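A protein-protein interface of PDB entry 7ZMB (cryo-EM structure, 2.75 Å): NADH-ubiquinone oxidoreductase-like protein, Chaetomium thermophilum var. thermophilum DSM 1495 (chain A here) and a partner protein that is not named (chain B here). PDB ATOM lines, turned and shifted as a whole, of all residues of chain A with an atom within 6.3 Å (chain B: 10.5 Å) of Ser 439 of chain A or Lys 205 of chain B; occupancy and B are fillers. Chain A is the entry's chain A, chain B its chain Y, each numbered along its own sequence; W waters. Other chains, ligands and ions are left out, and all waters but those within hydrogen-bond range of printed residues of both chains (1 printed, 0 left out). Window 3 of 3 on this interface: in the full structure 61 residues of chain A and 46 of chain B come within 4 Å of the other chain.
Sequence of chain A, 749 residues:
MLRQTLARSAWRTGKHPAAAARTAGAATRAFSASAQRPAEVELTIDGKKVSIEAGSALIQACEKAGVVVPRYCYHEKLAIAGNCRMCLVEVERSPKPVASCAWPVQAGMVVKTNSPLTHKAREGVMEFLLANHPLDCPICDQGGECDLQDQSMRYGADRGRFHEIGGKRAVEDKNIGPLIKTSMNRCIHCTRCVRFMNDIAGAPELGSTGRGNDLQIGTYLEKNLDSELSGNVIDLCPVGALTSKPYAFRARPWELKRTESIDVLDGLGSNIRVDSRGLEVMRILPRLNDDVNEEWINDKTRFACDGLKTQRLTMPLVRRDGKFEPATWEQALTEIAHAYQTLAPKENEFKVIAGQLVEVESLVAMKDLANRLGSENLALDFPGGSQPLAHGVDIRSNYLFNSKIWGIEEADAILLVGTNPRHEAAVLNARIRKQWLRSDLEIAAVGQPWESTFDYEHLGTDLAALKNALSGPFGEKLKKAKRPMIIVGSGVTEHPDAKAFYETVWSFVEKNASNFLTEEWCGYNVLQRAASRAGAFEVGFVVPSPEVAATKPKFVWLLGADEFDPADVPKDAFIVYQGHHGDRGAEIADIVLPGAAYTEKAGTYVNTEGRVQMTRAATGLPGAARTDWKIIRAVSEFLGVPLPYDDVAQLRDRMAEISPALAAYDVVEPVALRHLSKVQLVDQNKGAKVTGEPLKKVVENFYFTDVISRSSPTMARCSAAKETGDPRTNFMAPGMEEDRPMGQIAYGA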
ATOM      1  N   ALA A 411     -10.346  -9.857 -27.555  1.00  0.00           N
ATOM      2  CA  ALA A 411     -10.079  -8.483 -27.162  1.00  0.00           C
ATOM      3  C   ALA A 411     -10.912  -8.069 -25.955  1.00  0.00           C
ATOM      4  O   ALA A 411     -12.103  -8.371 -25.859  1.00  0.00           O
ATOM      5  CB  ALA A 411     -10.349  -7.553 -28.341  1.00  0.00           C
ATOM      6  N   ASP A 412     -10.266  -7.368 -25.025  1.00  0.00           N
ATOM      7  CA  ASP A 412     -10.900  -6.874 -23.813  1.00  0.00           C
ATOM      8  C   ASP A 412     -11.112  -5.375 -23.815  1.00  0.00           C
ATOM      9  O   ASP A 412     -12.115  -4.903 -23.284  1.00  0.00           O
ATOM     10  CB  ASP A 412     -10.060  -7.250 -22.590  1.00  0.00           C
ATOM     11  CG  ASP A 412     -10.067  -8.743 -22.315  1.00  0.00           C
ATOM     12  OD1 ASP A 412     -11.068  -9.411 -22.649  1.00  0.00           O
ATOM     13  OD2 ASP A 412      -9.064  -9.254 -21.772  1.00  0.00           O
ATOM     14  N   ARG A 433     -19.014  -6.512 -32.114  1.00  0.00           N
ATOM     15  CA  ARG A 433     -20.267  -6.612 -31.375  1.00  0.00           C
ATOM     16  C   ARG A 433     -20.423  -7.983 -30.731  1.00  0.00           C
ATOM     17  O   ARG A 433     -20.862  -8.090 -29.583  1.00  0.00           O
ATOM     18  CB  ARG A 433     -21.441  -6.311 -32.303  1.00  0.00           C
ATOM     19  CG  ARG A 433     -22.790  -6.662 -31.729  1.00  0.00           C
ATOM     20  CD  ARG A 433     -23.910  -6.187 -32.621  1.00  0.00           C
ATOM     21  NE  ARG A 433     -25.186  -6.756 -32.219  1.00  0.00           N
ATOM     22  CZ  ARG A 433     -26.022  -6.190 -31.360  1.00  0.00           C
ATOM     23  NH1 ARG A 433     -25.726  -5.029 -30.806  1.00  0.00           N
ATOM     24  NH2 ARG A 433     -27.159  -6.787 -31.058  1.00  0.00           N
ATOM     25  N   LYS A 434     -20.054  -9.042 -31.452  1.00  0.00           N
ATOM     26  CA  LYS A 434     -20.181 -10.393 -30.919  1.00  0.00           C
ATOM     27  C   LYS A 434     -19.343 -10.575 -29.661  1.00  0.00           C
ATOM     28  O   LYS A 434     -19.817 -11.128 -28.664  1.00  0.00           O
ATOM     29  CB  LYS A 434     -19.775 -11.402 -31.987  1.00  0.00           C
ATOM     30  CG  LYS A 434     -19.980 -12.836 -31.587  1.00  0.00           C
ATOM     31  CD  LYS A 434     -19.318 -13.751 -32.563  1.00  0.00           C
ATOM     32  CE  LYS A 434     -17.893 -13.341 -32.819  1.00  0.00           C
ATOM     33  NZ  LYS A 434     -17.361 -13.991 -34.026  1.00  0.00           N
ATOM     34  N   GLN A 435     -18.088 -10.121 -29.694  1.00  0.00           N
ATOM     35  CA  GLN A 435     -17.240 -10.179 -28.510  1.00  0.00           C
ATOM     36  C   GLN A 435     -17.792  -9.299 -27.398  1.00  0.00           C
ATOM     37  O   GLN A 435     -17.653  -9.621 -26.215  1.00  0.00           O
ATOM     38  CB  GLN A 435     -15.813  -9.768 -28.881  1.00  0.00           C
ATOM     39  CG  GLN A 435     -14.822  -9.585 -27.730  1.00  0.00           C
ATOM     40  CD  GLN A 435     -14.450 -10.863 -27.003  1.00  0.00           C
ATOM     41  OE1 GLN A 435     -15.247 -11.785 -26.869  1.00  0.00           O
ATOM     42  NE2 GLN A 435     -13.227 -10.914 -26.521  1.00  0.00           N
ATOM     43  N   TRP A 436     -18.428  -8.190 -27.764  1.00  0.00           N
ATOM     44  CA  TRP A 436     -18.939  -7.252 -26.776  1.00  0.00           C
ATOM     45  C   TRP A 436     -20.144  -7.816 -26.029  1.00  0.00           C
ATOM     46  O   TRP A 436     -20.278  -7.614 -24.818  1.00  0.00           O
ATOM     47  CB  TRP A 436     -19.282  -5.937 -27.471  1.00  0.00           C
ATOM     48  CG  TRP A 436     -20.007  -4.932 -26.646  1.00  0.00           C
ATOM     49  CD1 TRP A 436     -19.507  -4.201 -25.628  1.00  0.00           C
ATOM     50  CD2 TRP A 436     -21.365  -4.518 -26.810  1.00  0.00           C
ATOM     51  NE1 TRP A 436     -20.466  -3.358 -25.133  1.00  0.00           N
ATOM     52  CE2 TRP A 436     -21.619  -3.533 -25.845  1.00  0.00           C
ATOM     53  CE3 TRP A 436     -22.390  -4.882 -27.685  1.00  0.00           C
ATOM     54  CZ2 TRP A 436     -22.854  -2.916 -25.719  1.00  0.00           C
ATOM     55  CZ3 TRP A 436     -23.613  -4.262 -27.562  1.00  0.00           C
ATOM     56  CH2 TRP A 436     -23.835  -3.292 -26.588  1.00  0.00           C
ATOM     57  N   LEU A 437     -21.032  -8.524 -26.726  1.00  0.00           N
ATOM     58  CA  LEU A 437     -22.241  -9.019 -26.072  1.00  0.00           C
ATOM     59  C   LEU A 437     -21.922 -10.116 -25.073  1.00  0.00           C
ATOM     60  O   LEU A 437     -22.581 -10.228 -24.035  1.00  0.00           O
ATOM     61  CB  LEU A 437     -23.239  -9.538 -27.103  1.00  0.00           C
ATOM     62  CG  LEU A 437     -23.888  -8.593 -28.107  1.00  0.00           C
ATOM     63  CD1 LEU A 437     -24.336  -9.382 -29.302  1.00  0.00           C
ATOM     64  CD2 LEU A 437     -25.061  -7.876 -27.494  1.00  0.00           C
ATOM     65  N   ARG A 438     -20.921 -10.931 -25.366  1.00  0.00           N
ATOM     66  CA  ARG A 438     -20.608 -12.120 -24.592  1.00  0.00           C
ATOM     67  C   ARG A 438     -19.463 -11.923 -23.611  1.00  0.00           C
ATOM     68  O   ARG A 438     -19.007 -12.903 -23.018  1.00  0.00           O
ATOM     69  CB  ARG A 438     -20.270 -13.264 -25.539  1.00  0.00           C
ATOM     70  CG  ARG A 438     -18.938 -13.094 -26.208  1.00  0.00           C
ATOM     71  CD  ARG A 438     -18.711 -14.162 -27.233  1.00  0.00           C
ATOM     72  NE  ARG A 438     -17.420 -14.013 -27.884  1.00  0.00           N
ATOM     73  CZ  ARG A 438     -17.114 -14.560 -29.048  1.00  0.00           C
ATOM     74  NH1 ARG A 438     -18.005 -15.297 -29.686  1.00  0.00           N
ATOM     75  NH2 ARG A 438     -15.914 -14.376 -29.570  1.00  0.00           N
ATOM     76  N   SER A 439     -18.977 -10.703 -23.425  1.00  0.00           N
ATOM     77  CA  SER A 439     -17.805 -10.497 -22.586  1.00  0.00           C
ATOM     78  C   SER A 439     -17.806  -9.067 -22.073  1.00  0.00           C
ATOM     79  O   SER A 439     -18.668  -8.261 -22.422  1.00  0.00           O
ATOM     80  CB  SER A 439     -16.515 -10.811 -23.346  1.00  0.00           C
ATOM     81  OG  SER A 439     -16.118  -9.719 -24.147  1.00  0.00           O
ATOM     82  N   ASP A 440     -16.828  -8.764 -21.225  1.00  0.00           N
ATOM     83  CA  ASP A 440     -16.671  -7.431 -20.647  1.00  0.00           C
ATOM     84  C   ASP A 440     -15.743  -6.557 -21.487  1.00  0.00           C
ATOM     85  O   ASP A 440     -14.796  -5.957 -20.985  1.00  0.00           O
ATOM     86  CB  ASP A 440     -16.168  -7.550 -19.216  1.00  0.00           C
ATOM     87  CG  ASP A 440     -17.198  -8.160 -18.289  1.00  0.00           C
ATOM     88  OD1 ASP A 440     -18.386  -8.205 -18.669  1.00  0.00           O
ATOM     89  OD2 ASP A 440     -16.819  -8.594 -17.182  1.00  0.00           O
ATOM     90  N   LEU A 441     -16.022  -6.474 -22.782  1.00  0.00           N
ATOM     91  CA  LEU A 441     -15.210  -5.679 -23.687  1.00  0.00           C
ATOM     92  C   LEU A 441     -15.616  -4.213 -23.609  1.00  0.00           C
ATOM     93  O   LEU A 441     -16.802  -3.879 -23.682  1.00  0.00           O
ATOM     94  CB  LEU A 441     -15.354  -6.198 -25.115  1.00  0.00           C
ATOM     95  CG  LEU A 441     -15.010  -5.257 -26.264  1.00  0.00           C
ATOM     96  CD1 LEU A 441     -13.521  -4.913 -26.306  1.00  0.00           C
ATOM     97  CD2 LEU A 441     -15.463  -5.866 -27.573  1.00  0.00           C
ATOM     98  N   GLU A 442     -14.628  -3.340 -23.466  1.00  0.00           N
ATOM     99  CA  GLU A 442     -14.842  -1.904 -23.395  1.00  0.00           C
ATOM    100  C   GLU A 442     -14.288  -1.256 -24.650  1.00  0.00           C
ATOM    101  O   GLU A 442     -13.142  -1.504 -25.025  1.00  0.00           O
ATOM    102  CB  GLU A 442     -14.177  -1.319 -22.149  1.00  0.00           C
ATOM    103  CG  GLU A 442     -14.843  -1.734 -20.846  1.00  0.00           C
ATOM    104  CD  GLU A 442     -16.333  -1.464 -20.845  1.00  0.00           C
ATOM    105  OE1 GLU A 442     -16.755  -0.432 -21.411  1.00  0.00           O
ATOM    106  OE2 GLU A 442     -17.088  -2.286 -20.286  1.00  0.00           O
ATOM    107  N   ARG B 189     -16.589 -23.970 -30.810  1.00  0.00           N
ATOM    108  CA  ARG B 189     -16.972 -23.194 -29.645  1.00  0.00           C
ATOM    109  C   ARG B 189     -18.209 -23.840 -29.048  1.00  0.00           C
ATOM    110  O   ARG B 189     -19.169 -24.118 -29.771  1.00  0.00           O
ATOM    111  CB  ARG B 189     -17.247 -21.740 -30.023  1.00  0.00           C
ATOM    112  CG  ARG B 189     -17.584 -20.842 -28.863  1.00  0.00           C
ATOM    113  CD  ARG B 189     -17.663 -19.404 -29.305  1.00  0.00           C
ATOM    114  NE  ARG B 189     -17.920 -18.516 -28.182  1.00  0.00           N
ATOM    115  CZ  ARG B 189     -16.987 -17.807 -27.562  1.00  0.00           C
ATOM    116  NH1 ARG B 189     -17.312 -17.030 -26.543  1.00  0.00           N
ATOM    117  NH2 ARG B 189     -15.729 -17.870 -27.965  1.00  0.00           N
ATOM    118  N   ASN B 195     -27.277 -19.824 -22.424  1.00  0.00           N
ATOM    119  CA  ASN B 195     -26.733 -18.484 -22.641  1.00  0.00           C
ATOM    120  C   ASN B 195     -27.810 -17.489 -23.032  1.00  0.00           C
ATOM    121  O   ASN B 195     -27.650 -16.287 -22.793  1.00  0.00           O
ATOM    122  CB  ASN B 195     -25.636 -18.464 -23.711  1.00  0.00           C
ATOM    123  CG  ASN B 195     -24.413 -19.256 -23.326  1.00  0.00           C
ATOM    124  OD1 ASN B 195     -24.082 -20.255 -23.953  1.00  0.00           O
ATOM    125  ND2 ASN B 195     -23.745 -18.823 -22.271  1.00  0.00           N
ATOM    126  N   LEU B 198     -28.913 -15.616 -19.635  1.00  0.00           N
ATOM    127  CA  LEU B 198     -27.967 -15.351 -18.569  1.00  0.00           C
ATOM    128  C   LEU B 198     -28.336 -14.074 -17.829  1.00  0.00           C
ATOM    129  O   LEU B 198     -28.865 -13.119 -18.405  1.00  0.00           O
ATOM    130  CB  LEU B 198     -26.550 -15.250 -19.120  1.00  0.00           C
ATOM    131  CG  LEU B 198     -26.017 -16.517 -19.781  1.00  0.00           C
ATOM    132  CD1 LEU B 198     -24.576 -16.328 -20.216  1.00  0.00           C
ATOM    133  CD2 LEU B 198     -26.152 -17.734 -18.861  1.00  0.00           C
ATOM    134  N   TYR B 199     -28.074 -14.079 -16.529  1.00  0.00           N
ATOM    135  CA  TYR B 199     -28.369 -12.926 -15.703  1.00  0.00           C
ATOM    136  C   TYR B 199     -27.444 -11.775 -16.063  1.00  0.00           C
ATOM    137  O   TYR B 199     -26.279 -11.976 -16.407  1.00  0.00           O
ATOM    138  CB  TYR B 199     -28.219 -13.292 -14.230  1.00  0.00           C
ATOM    139  CG  TYR B 199     -28.302 -12.124 -13.287  1.00  0.00           C
ATOM    140  CD1 TYR B 199     -29.523 -11.535 -12.994  1.00  0.00           C
ATOM    141  CD2 TYR B 199     -27.167 -11.616 -12.677  1.00  0.00           C
ATOM    142  CE1 TYR B 199     -29.610 -10.482 -12.136  1.00  0.00           C
ATOM    143  CE2 TYR B 199     -27.251 -10.552 -11.809  1.00  0.00           C
ATOM    144  CZ  TYR B 199     -28.475  -9.991 -11.544  1.00  0.00           C
ATOM    145  OH  TYR B 199     -28.571  -8.932 -10.681  1.00  0.00           O
ATOM    146  N   SER B 200     -27.976 -10.566 -16.002  1.00  0.00           N
ATOM    147  CA  SER B 200     -27.191  -9.362 -16.247  1.00  0.00           C
ATOM    148  C   SER B 200     -27.256  -8.483 -15.013  1.00  0.00           C
ATOM    149  O   SER B 200     -28.339  -7.964 -14.683  1.00  0.00           O
ATOM    150  CB  SER B 200     -27.701  -8.605 -17.472  1.00  0.00           C
ATOM    151  OG  SER B 200     -27.104  -7.326 -17.554  1.00  0.00           O
ATOM    152  N   PRO B 201     -26.151  -8.311 -14.286  1.00  0.00           N
ATOM    153  CA  PRO B 201     -26.171  -7.414 -13.126  1.00  0.00           C
ATOM    154  C   PRO B 201     -26.282  -5.951 -13.502  1.00  0.00           C
ATOM    155  O   PRO B 201     -26.722  -5.151 -12.672  1.00  0.00           O
ATOM    156  CB  PRO B 201     -24.837  -7.709 -12.429  1.00  0.00           C
ATOM    157  CG  PRO B 201     -24.271  -8.912 -13.124  1.00  0.00           C
ATOM    158  CD  PRO B 201     -24.829  -8.910 -14.493  1.00  0.00           C
ATOM    159  N   GLY B 202     -25.909  -5.578 -14.720  1.00  0.00           N
ATOM    160  CA  GLY B 202     -25.997  -4.202 -15.146  1.00  0.00           C
ATOM    161  C   GLY B 202     -26.829  -3.991 -16.391  1.00  0.00           C
ATOM    162  O   GLY B 202     -27.803  -4.707 -16.630  1.00  0.00           O
ATOM    163  N   LYS B 203     -26.444  -3.008 -17.198  1.00  0.00           N
ATOM    164  CA  LYS B 203     -27.253  -2.604 -18.338  1.00  0.00           C
ATOM    165  C   LYS B 203     -27.365  -3.730 -19.354  1.00  0.00           C
ATOM    166  O   LYS B 203     -26.368  -4.353 -19.724  1.00  0.00           O
ATOM    167  CB  LYS B 203     -26.645  -1.363 -18.986  1.00  0.00           C
ATOM    168  CG  LYS B 203     -27.565  -0.625 -19.923  1.00  0.00           C
ATOM    169  CD  LYS B 203     -26.903   0.644 -20.422  1.00  0.00           C
ATOM    170  CE  LYS B 203     -27.713   1.301 -21.524  1.00  0.00           C
ATOM    171  NZ  LYS B 203     -27.061   2.548 -22.006  1.00  0.00           N
ATOM    172  N   LEU B 204     -28.587  -3.993 -19.806  1.00  0.00           N
ATOM    173  CA  LEU B 204     -28.796  -5.000 -20.838  1.00  0.00           C
ATOM    174  C   LEU B 204     -28.230  -4.493 -22.156  1.00  0.00           C
ATOM    175  O   LEU B 204     -28.691  -3.480 -22.689  1.00  0.00           O
ATOM    176  CB  LEU B 204     -30.280  -5.323 -20.977  1.00  0.00           C
ATOM    177  CG  LEU B 204     -31.063  -5.691 -19.717  1.00  0.00           C
ATOM    178  CD1 LEU B 204     -32.419  -6.242 -20.105  1.00  0.00           C
ATOM    179  CD2 LEU B 204     -30.310  -6.683 -18.884  1.00  0.00           C
ATOM    180  N   LYS B 205     -27.226  -5.191 -22.682  1.00  0.00           N
ATOM    181  CA  LYS B 205     -26.542  -4.698 -23.871  1.00  0.00           C
ATOM    182  C   LYS B 205     -27.384  -4.904 -25.128  1.00  0.00           C
ATOM    183  O   LYS B 205     -27.263  -4.137 -26.090  1.00  0.00           O
ATOM    184  CB  LYS B 205     -25.172  -5.356 -23.991  1.00  0.00           C
ATOM    185  CG  LYS B 205     -24.422  -5.343 -22.684  1.00  0.00           C
ATOM    186  CD  LYS B 205     -23.217  -6.241 -22.684  1.00  0.00           C
ATOM    187  CE  LYS B 205     -21.968  -5.455 -23.011  1.00  0.00           C
ATOM    188  NZ  LYS B 205     -20.738  -6.251 -22.770  1.00  0.00           N
ATOM    189  N   HIS B 206     -28.240  -5.921 -25.145  1.00  0.00           N
ATOM    190  CA  HIS B 206     -29.300  -5.988 -26.141  1.00  0.00           C
ATOM    191  C   HIS B 206     -30.471  -6.769 -25.577  1.00  0.00           C
ATOM    192  O   HIS B 206     -30.343  -7.511 -24.603  1.00  0.00           O
ATOM    193  CB  HIS B 206     -28.825  -6.593 -27.476  1.00  0.00           C
ATOM    194  CG  HIS B 206     -28.858  -8.086 -27.530  1.00  0.00           C
ATOM    195  ND1 HIS B 206     -28.126  -8.880 -26.675  1.00  0.00           N
ATOM    196  CD2 HIS B 206     -29.501  -8.929 -28.368  1.00  0.00           C
ATOM    197  CE1 HIS B 206     -28.334 -10.149 -26.973  1.00  0.00           C
ATOM    198  NE2 HIS B 206     -29.166 -10.206 -27.996  1.00  0.00           N
ATOM    199  N   ILE B 207     -31.628  -6.570 -26.187  1.00  0.00           N
ATOM    200  CA  ILE B 207     -32.859  -7.212 -25.764  1.00  0.00           C
ATOM    201  C   ILE B 207     -33.095  -8.379 -26.711  1.00  0.00           C
ATOM    202  O   ILE B 207     -33.420  -8.190 -27.887  1.00  0.00           O
ATOM    203  CB  ILE B 207     -34.034  -6.232 -25.738  1.00  0.00           C
ATOM    204  CG1 ILE B 207     -33.866  -5.278 -24.560  1.00  0.00           C
ATOM    205  CG2 ILE B 207     -35.345  -6.974 -25.606  1.00  0.00           C
ATOM    206  CD1 ILE B 207     -34.381  -3.896 -24.801  1.00  0.00           C
ATOM    207  N   ARG B 208     -32.914  -9.592 -26.199  1.00  0.00           N
ATOM    208  CA  ARG B 208     -33.051 -10.787 -27.015  1.00  0.00           C
ATOM    209  C   ARG B 208     -34.514 -11.038 -27.366  1.00  0.00           C
ATOM    210  O   ARG B 208     -35.425 -10.721 -26.599  1.00  0.00           O
ATOM    211  CB  ARG B 208     -32.455 -11.986 -26.286  1.00  0.00           C
ATOM    212  CG  ARG B 208     -32.160 -13.159 -27.185  1.00  0.00           C
ATOM    213  CD  ARG B 208     -31.549 -14.300 -26.409  1.00  0.00           C
ATOM    214  NE  ARG B 208     -30.289 -13.899 -25.806  1.00  0.00           N
ATOM    215  CZ  ARG B 208     -29.102 -14.111 -26.355  1.00  0.00           C
ATOM    216  NH1 ARG B 208     -28.007 -13.707 -25.733  1.00  0.00           N
ATOM    217  NH2 ARG B 208     -29.013 -14.720 -27.525  1.00  0.00           N
HETATM  218  O   HOH W   1     -27.390  -4.043 -28.633  1.00  0.00           O
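Among the printed residues, merely in contact across the chains: Leu 437 of chain A with His 206 of chain B (3.3 Å) and Arg 433 of chain A with His 206 of chain B (3.96 Å).
Water W1 bridges O of Lys 205 of chain B (2.5 Å) and NH1 of Arg 433 of chain A (2.9 Å).
Of the 13 printed residues of chain B, 3 touch a printed residue of chain A. Printed residues of chain A that touch a printed residue of chain B: Arg 433, Trp 436, Leu 437, Arg 438 and Ser 439. Hydrophobic or aromatic side chains of chain A within 4 Å of the printed part of chain B: Trp 436 and Leu 437. Among the printed residues, no Asp or Glu carboxylate lies within 4 Å of a Lys or Arg side-chain nitrogen of the other chain.
The backbone carbonyl oxygen (O) of Trp 436 of chain A sits at hydrogen-bond distance from the side-chain amino group (NZ) of Lys 205 of chain B (2.5 Å). NE of Arg 438 of chain A lies close to NH1 of Arg 189 of chain B (3.3 Å). The side-chain amino group of Lys 205 of chain B lies within hydrogen-bond range of the backbone carbonyl oxygen of Ser 439 of chain A (2.9 Å).
Printed residues of chain B within 4 Å of Arg 433 of chain A: His 206. No residue of chain B comes within 4 Å of Gln 435 of chain A. Of the printed residues of chain B, Trp 436 of chain A touches Lys 205 (2.5 Å). Of the printed residues of chain B, Leu 437 of chain A touches His 206 (3.3 Å). Of the printed residues of chain B, Arg 438 of chain A touches Arg 189. Ser 439 of chain A touches just one residue of chain B: Lys 205 (2.9 Å). No residue of chain B comes within 4 Å of Asp 440 of chain A. Printed residues of chain A within 4 Å of Arg 189 of chain B: Arg 438 (3.3 Å). Lys 205 of chain B touches just these residues of chain A: Trp 436 and Ser 439. Of the printed residues of chain A, His 206 of chain B touches Arg 433 and Leu 437.
The guanidinium group of Arg 438 of chain A sits at hydrogen-bond distance from the side-chain amide oxygen of Gln 435 of chain A (3.3 Å). The backbone carbonyl oxygen (O) of Gln 435 of chain A is in hydrogen-bond range of the side-chain hydroxyl (OG) of Ser 439 of chain A (2.6 Å).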
